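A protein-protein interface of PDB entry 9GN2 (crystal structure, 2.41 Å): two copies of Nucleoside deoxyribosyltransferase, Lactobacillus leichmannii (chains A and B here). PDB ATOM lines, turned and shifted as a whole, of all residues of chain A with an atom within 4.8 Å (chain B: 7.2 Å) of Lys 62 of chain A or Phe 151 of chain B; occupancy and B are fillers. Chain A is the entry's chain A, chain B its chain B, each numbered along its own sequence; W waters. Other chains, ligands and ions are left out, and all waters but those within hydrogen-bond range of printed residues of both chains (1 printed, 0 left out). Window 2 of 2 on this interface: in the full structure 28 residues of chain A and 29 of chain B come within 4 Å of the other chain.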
ATOM      1  N   HIS A  60      -7.714  -5.094   6.824  1.00  0.00           N
ATOM      2  CA  HIS A  60      -7.470  -4.205   5.697  1.00  0.00           C
ATOM      3  C   HIS A  60      -6.847  -2.893   6.169  1.00  0.00           C
ATOM      4  O   HIS A  60      -6.353  -2.173   5.304  1.00  0.00           O
ATOM      5  CB  HIS A  60      -8.705  -4.053   4.792  1.00  0.00           C
ATOM      6  CG  HIS A  60      -9.029  -5.223   3.883  1.00  0.00           C
ATOM      7  ND1 HIS A  60      -9.919  -6.220   4.250  1.00  0.00           N
ATOM      8  CD2 HIS A  60      -8.647  -5.538   2.619  1.00  0.00           C
ATOM      9  CE1 HIS A  60     -10.053  -7.107   3.251  1.00  0.00           C
ATOM     10  NE2 HIS A  60      -9.290  -6.715   2.248  1.00  0.00           N
ATOM     11  N   ASP A  61      -6.799  -2.634   7.502  1.00  0.00           N
ATOM     12  CA  ASP A  61      -6.104  -1.496   8.092  1.00  0.00           C
ATOM     13  C   ASP A  61      -4.583  -1.521   7.823  1.00  0.00           C
ATOM     14  O   ASP A  61      -3.845  -2.379   8.308  1.00  0.00           O
ATOM     15  CB  ASP A  61      -6.414  -1.358   9.574  1.00  0.00           C
ATOM     16  CG  ASP A  61      -5.845  -0.122  10.268  1.00  0.00           C
ATOM     17  OD1 ASP A  61      -5.102   0.615   9.601  1.00  0.00           O
ATOM     18  OD2 ASP A  61      -6.119   0.102  11.488  1.00  0.00           O
ATOM     19  N   LYS A  62      -4.106  -0.538   7.046  1.00  0.00           N
ATOM     20  CA  LYS A  62      -2.719  -0.492   6.613  1.00  0.00           C
ATOM     21  C   LYS A  62      -1.858   0.135   7.710  1.00  0.00           C
ATOM     22  O   LYS A  62      -0.648  -0.064   7.763  1.00  0.00           O
ATOM     23  CB  LYS A  62      -2.553   0.293   5.307  1.00  0.00           C
ATOM     24  CG  LYS A  62      -3.040  -0.425   4.048  1.00  0.00           C
ATOM     25  CD  LYS A  62      -2.889   0.484   2.839  1.00  0.00           C
ATOM     26  CE  LYS A  62      -3.335  -0.099   1.543  1.00  0.00           C
ATOM     27  NZ  LYS A  62      -4.797  -0.084   1.473  1.00  0.00           N
ATOM     28  N   VAL A  63      -2.482   0.892   8.602  1.00  0.00           N
ATOM     29  CA  VAL A  63      -1.769   1.459   9.734  1.00  0.00           C
ATOM     30  C   VAL A  63      -1.387   0.329  10.695  1.00  0.00           C
ATOM     31  O   VAL A  63      -0.219   0.219  11.070  1.00  0.00           O
ATOM     32  CB  VAL A  63      -2.632   2.535  10.416  1.00  0.00           C
ATOM     33  CG1 VAL A  63      -2.017   3.047  11.719  1.00  0.00           C
ATOM     34  CG2 VAL A  63      -2.929   3.698   9.462  1.00  0.00           C
ATOM     35  N   TRP A  64      -2.380  -0.492  11.078  1.00  0.00           N
ATOM     36  CA  TRP A  64      -2.129  -1.638  11.930  1.00  0.00           C
ATOM     37  C   TRP A  64      -1.016  -2.494  11.324  1.00  0.00           C
ATOM     38  O   TRP A  64      -0.056  -2.765  12.021  1.00  0.00           O
ATOM     39  CB  TRP A  64      -3.401  -2.461  12.205  1.00  0.00           C
ATOM     40  CG  TRP A  64      -3.111  -3.683  13.042  1.00  0.00           C
ATOM     41  CD1 TRP A  64      -3.058  -3.786  14.404  1.00  0.00           C
ATOM     42  CD2 TRP A  64      -2.760  -4.975  12.519  1.00  0.00           C
ATOM     43  NE1 TRP A  64      -2.721  -5.064  14.768  1.00  0.00           N
ATOM     44  CE2 TRP A  64      -2.530  -5.811  13.627  1.00  0.00           C
ATOM     45  CE3 TRP A  64      -2.631  -5.495  11.226  1.00  0.00           C
ATOM     46  CZ2 TRP A  64      -2.163  -7.139  13.465  1.00  0.00           C
ATOM     47  CZ3 TRP A  64      -2.252  -6.807  11.065  1.00  0.00           C
ATOM     48  CH2 TRP A  64      -2.013  -7.613  12.177  1.00  0.00           C
ATOM     49  N   ALA A  65      -1.119  -2.838  10.034  1.00  0.00           N
ATOM     50  CA  ALA A  65      -0.142  -3.670   9.362  1.00  0.00           C
ATOM     51  C   ALA A  65       1.244  -3.031   9.365  1.00  0.00           C
ATOM     52  O   ALA A  65       2.228  -3.733   9.602  1.00  0.00           O
ATOM     53  CB  ALA A  65      -0.586  -3.961   7.946  1.00  0.00           C
ATOM     54  N   THR A  66       1.320  -1.719   9.084  1.00  0.00           N
ATOM     55  CA  THR A  66       2.605  -1.028   9.013  1.00  0.00           C
ATOM     56  C   THR A  66       3.295  -1.082  10.373  1.00  0.00           C
ATOM     57  O   THR A  66       4.458  -1.465  10.467  1.00  0.00           O
ATOM     58  CB  THR A  66       2.488   0.419   8.538  1.00  0.00           C
ATOM     59  OG1 THR A  66       1.978   0.426   7.208  1.00  0.00           O
ATOM     60  CG2 THR A  66       3.844   1.100   8.486  1.00  0.00           C
ATOM     61  N   TYR B 118      -5.838 -12.928  -6.424  1.00  0.00           N
ATOM     62  CA  TYR B 118      -5.482 -11.589  -5.973  1.00  0.00           C
ATOM     63  C   TYR B 118      -6.604 -11.039  -5.088  1.00  0.00           C
ATOM     64  O   TYR B 118      -7.746 -11.054  -5.479  1.00  0.00           O
ATOM     65  CB  TYR B 118      -5.179 -10.648  -7.140  1.00  0.00           C
ATOM     66  CG  TYR B 118      -4.442  -9.378  -6.730  1.00  0.00           C
ATOM     67  CD1 TYR B 118      -5.107  -8.299  -6.160  1.00  0.00           C
ATOM     68  CD2 TYR B 118      -3.069  -9.251  -6.936  1.00  0.00           C
ATOM     69  CE1 TYR B 118      -4.429  -7.148  -5.790  1.00  0.00           C
ATOM     70  CE2 TYR B 118      -2.381  -8.103  -6.564  1.00  0.00           C
ATOM     71  CZ  TYR B 118      -3.065  -7.052  -5.975  1.00  0.00           C
ATOM     72  OH  TYR B 118      -2.419  -5.910  -5.579  1.00  0.00           O
ATOM     73  N   TRP B 127       3.523  -9.201   3.040  1.00  0.00           N
ATOM     74  CA  TRP B 127       3.028  -7.868   2.769  1.00  0.00           C
ATOM     75  C   TRP B 127       4.118  -6.818   2.999  1.00  0.00           C
ATOM     76  O   TRP B 127       4.319  -5.929   2.178  1.00  0.00           O
ATOM     77  CB  TRP B 127       1.799  -7.652   3.660  1.00  0.00           C
ATOM     78  CG  TRP B 127       1.220  -6.270   3.573  1.00  0.00           C
ATOM     79  CD1 TRP B 127       0.246  -5.829   2.732  1.00  0.00           C
ATOM     80  CD2 TRP B 127       1.571  -5.154   4.409  1.00  0.00           C
ATOM     81  NE1 TRP B 127       0.013  -4.505   2.945  1.00  0.00           N
ATOM     82  CE2 TRP B 127       0.793  -4.067   3.979  1.00  0.00           C
ATOM     83  CE3 TRP B 127       2.464  -4.963   5.461  1.00  0.00           C
ATOM     84  CZ2 TRP B 127       0.876  -2.821   4.586  1.00  0.00           C
ATOM     85  CZ3 TRP B 127       2.539  -3.727   6.066  1.00  0.00           C
ATOM     86  CH2 TRP B 127       1.762  -2.668   5.625  1.00  0.00           C
ATOM     87  N   SER B 130       7.577  -7.018   0.804  1.00  0.00           N
ATOM     88  CA  SER B 130       7.312  -6.647  -0.572  1.00  0.00           C
ATOM     89  C   SER B 130       7.425  -5.125  -0.723  1.00  0.00           C
ATOM     90  O   SER B 130       6.977  -4.363   0.138  1.00  0.00           O
ATOM     91  CB  SER B 130       5.969  -7.164  -1.020  1.00  0.00           C
ATOM     92  OG  SER B 130       4.919  -6.310  -0.572  1.00  0.00           O
ATOM     93  N   ASP B 131       8.010  -4.713  -1.845  1.00  0.00           N
ATOM     94  CA  ASP B 131       7.877  -3.340  -2.300  1.00  0.00           C
ATOM     95  C   ASP B 131       6.564  -3.124  -3.069  1.00  0.00           C
ATOM     96  O   ASP B 131       6.020  -2.015  -3.098  1.00  0.00           O
ATOM     97  CB  ASP B 131       9.102  -2.963  -3.100  1.00  0.00           C
ATOM     98  CG  ASP B 131      10.383  -2.900  -2.281  1.00  0.00           C
ATOM     99  OD1 ASP B 131      10.395  -2.158  -1.276  1.00  0.00           O
ATOM    100  OD2 ASP B 131      11.368  -3.555  -2.700  1.00  0.00           O
ATOM    101  N   ASN B 132       6.009  -4.202  -3.634  1.00  0.00           N
ATOM    102  CA  ASN B 132       4.789  -4.090  -4.413  1.00  0.00           C
ATOM    103  C   ASN B 132       4.234  -5.488  -4.632  1.00  0.00           C
ATOM    104  O   ASN B 132       5.007  -6.455  -4.712  1.00  0.00           O
ATOM    105  CB  ASN B 132       5.081  -3.379  -5.736  1.00  0.00           C
ATOM    106  CG  ASN B 132       3.862  -2.961  -6.540  1.00  0.00           C
ATOM    107  OD1 ASN B 132       4.012  -2.576  -7.703  1.00  0.00           O
ATOM    108  ND2 ASN B 132       2.661  -2.952  -5.983  1.00  0.00           N
ATOM    109  N   VAL B 133       2.905  -5.588  -4.762  1.00  0.00           N
ATOM    110  CA  VAL B 133       2.346  -6.857  -5.195  1.00  0.00           C
ATOM    111  C   VAL B 133       1.265  -6.654  -6.261  1.00  0.00           C
ATOM    112  O   VAL B 133       0.359  -5.844  -6.121  1.00  0.00           O
ATOM    113  CB  VAL B 133       1.972  -7.722  -3.962  1.00  0.00           C
ATOM    114  CG1 VAL B 133       2.081  -6.961  -2.642  1.00  0.00           C
ATOM    115  CG2 VAL B 133       0.673  -8.503  -4.091  1.00  0.00           C
ATOM    116  N   PHE B 149       6.933   1.667  -5.212  1.00  0.00           N
ATOM    117  CA  PHE B 149       6.359   1.117  -3.995  1.00  0.00           C
ATOM    118  C   PHE B 149       4.838   1.251  -4.023  1.00  0.00           C
ATOM    119  O   PHE B 149       4.334   2.358  -4.172  1.00  0.00           O
ATOM    120  CB  PHE B 149       6.832   1.853  -2.726  1.00  0.00           C
ATOM    121  CG  PHE B 149       6.206   1.264  -1.470  1.00  0.00           C
ATOM    122  CD1 PHE B 149       6.801   0.186  -0.823  1.00  0.00           C
ATOM    123  CD2 PHE B 149       4.989   1.745  -0.976  1.00  0.00           C
ATOM    124  CE1 PHE B 149       6.214  -0.378   0.303  1.00  0.00           C
ATOM    125  CE2 PHE B 149       4.395   1.166   0.135  1.00  0.00           C
ATOM    126  CZ  PHE B 149       5.014   0.110   0.773  1.00  0.00           C
ATOM    127  N   ASP B 150       4.115   0.171  -3.703  1.00  0.00           N
ATOM    128  CA  ASP B 150       2.682   0.281  -3.483  1.00  0.00           C
ATOM    129  C   ASP B 150       2.219  -0.859  -2.573  1.00  0.00           C
ATOM    130  O   ASP B 150       2.913  -1.856  -2.421  1.00  0.00           O
ATOM    131  CB  ASP B 150       1.946   0.325  -4.820  1.00  0.00           C
ATOM    132  CG  ASP B 150       0.516   0.844  -4.819  1.00  0.00           C
ATOM    133  OD1 ASP B 150       0.040   1.323  -3.750  1.00  0.00           O
ATOM    134  OD2 ASP B 150      -0.105   0.777  -5.910  1.00  0.00           O
ATOM    135  N   PHE B 151       1.010  -0.719  -2.023  1.00  0.00           N
ATOM    136  CA  PHE B 151       0.407  -1.700  -1.139  1.00  0.00           C
ATOM    137  C   PHE B 151      -0.460  -2.686  -1.921  1.00  0.00           C
ATOM    138  O   PHE B 151      -1.138  -2.316  -2.884  1.00  0.00           O
ATOM    139  CB  PHE B 151      -0.484  -0.987  -0.127  1.00  0.00           C
ATOM    140  CG  PHE B 151       0.223  -0.074   0.864  1.00  0.00           C
ATOM    141  CD1 PHE B 151       1.011  -0.595   1.885  1.00  0.00           C
ATOM    142  CD2 PHE B 151       0.051   1.302   0.819  1.00  0.00           C
ATOM    143  CE1 PHE B 151       1.650   0.239   2.804  1.00  0.00           C
ATOM    144  CE2 PHE B 151       0.689   2.131   1.742  1.00  0.00           C
ATOM    145  CZ  PHE B 151       1.482   1.598   2.736  1.00  0.00           C
ATOM    146  N   TYR B 152      -0.446  -3.946  -1.473  1.00  0.00           N
ATOM    147  CA  TYR B 152      -1.413  -4.958  -1.887  1.00  0.00           C
ATOM    148  C   TYR B 152      -2.842  -4.455  -1.715  1.00  0.00           C
ATOM    149  O   TYR B 152      -3.155  -3.808  -0.716  1.00  0.00           O
ATOM    150  CB  TYR B 152      -1.211  -6.191  -1.010  1.00  0.00           C
ATOM    151  CG  TYR B 152      -1.997  -7.456  -1.318  1.00  0.00           C
ATOM    152  CD1 TYR B 152      -2.243  -7.880  -2.618  1.00  0.00           C
ATOM    153  CD2 TYR B 152      -2.462  -8.261  -0.279  1.00  0.00           C
ATOM    154  CE1 TYR B 152      -2.930  -9.063  -2.869  1.00  0.00           C
ATOM    155  CE2 TYR B 152      -3.150  -9.442  -0.511  1.00  0.00           C
ATOM    156  CZ  TYR B 152      -3.387  -9.842  -1.815  1.00  0.00           C
ATOM    157  OH  TYR B 152      -4.062 -11.007  -2.033  1.00  0.00           O
ATOM    158  N   GLU B 153      -3.671  -4.715  -2.732  1.00  0.00           N
ATOM    159  CA  GLU B 153      -5.098  -4.421  -2.682  1.00  0.00           C
ATOM    160  C   GLU B 153      -5.779  -5.720  -2.251  1.00  0.00           C
ATOM    161  O   GLU B 153      -6.320  -6.471  -3.082  1.00  0.00           O
ATOM    162  CB  GLU B 153      -5.679  -3.885  -4.002  1.00  0.00           C
ATOM    163  CG  GLU B 153      -5.152  -2.537  -4.495  1.00  0.00           C
ATOM    164  CD  GLU B 153      -5.730  -2.180  -5.866  1.00  0.00           C
ATOM    165  OE1 GLU B 153      -6.900  -1.735  -5.886  1.00  0.00           O
ATOM    166  OE2 GLU B 153      -5.058  -2.394  -6.911  1.00  0.00           O
ATOM    167  N   GLY B 154      -5.702  -6.005  -0.942  1.00  0.00           N
ATOM    168  CA  GLY B 154      -6.028  -7.334  -0.458  1.00  0.00           C
ATOM    169  C   GLY B 154      -5.857  -7.433   1.044  1.00  0.00           C
ATOM    170  O   GLY B 154      -5.431  -6.484   1.688  1.00  0.00           O
ATOM    171  N   VAL B 156      -4.527  -9.001   4.775  1.00  0.00           N
ATOM    172  CA  VAL B 156      -3.303  -9.539   5.346  1.00  0.00           C
ATOM    173  C   VAL B 156      -3.559 -10.016   6.781  1.00  0.00           C
ATOM    174  O   VAL B 156      -4.095  -9.259   7.587  1.00  0.00           O
ATOM    175  CB  VAL B 156      -2.154  -8.514   5.171  1.00  0.00           C
ATOM    176  CG1 VAL B 156      -2.595  -7.128   4.712  1.00  0.00           C
ATOM    177  CG2 VAL B 156      -1.278  -8.405   6.400  1.00  0.00           C
HETATM  178  O   HOH W   1      -4.453  -4.285   4.205  1.00  0.00           O
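Water W1 lies within hydrogen-bond range of O of His 60 of chain A (3.0 Å) and O of Gly 154 of chain B (3.5 Å).
Phe 151 of chain B touches one residue of chain A. Printed residues of chain A within 4 Å of Gly 154 of chain B: His 60. Of the printed residues of chain B, Ala 65 of chain A touches Trp 127 (3.5 Å). Printed residues of chain A within 4 Å of Trp 127 of chain B: Ala 65 and Thr 66. Printed residues of chain B within 4 Å of His 60 of chain A: Gly 154 (3.5 Å). The nearest printed residue of chain A that does not touch Gly 154 of chain B is Lys 62 of chain A (6.4 Å).
The side-chain hydroxyl (OG1) of Thr 66 of chain A lies within hydrogen-bond range of the backbone carbonyl oxygen (O) of Lys 62 of chain A (2.7 Å). The backbone carbonyl oxygen (O) of Trp 127 of chain B sits at hydrogen-bond distance from the side-chain hydroxyl (OG) of Ser 130 of chain B (2.8 Å).
Among the printed residues, merely in contact across the chains: Lys 62 of chain A with Phe 151 of chain B (3.4 Å), His 60 of chain A with Gly 154 of chain B (3.5 Å), Thr 66 of chain A with Trp 127 of chain B (3.5 Å) and Ala 65 of chain A with Trp 127 of chain B (3.5 Å).
No position is printed for both chains.
Hydrophobic or aromatic side chains of chain A that line the printed part of chain B: His 60 and Ala 65. Printed residues of chain B that touch a printed residue of chain A: Trp 127, Phe 151 and Gly 154. Among the printed residues, 4 pairs touch across the chains. Among the printed residues, no Asp or Glu carboxylate lies within 4 Å of a Lys or Arg side-chain nitrogen of the other chain.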
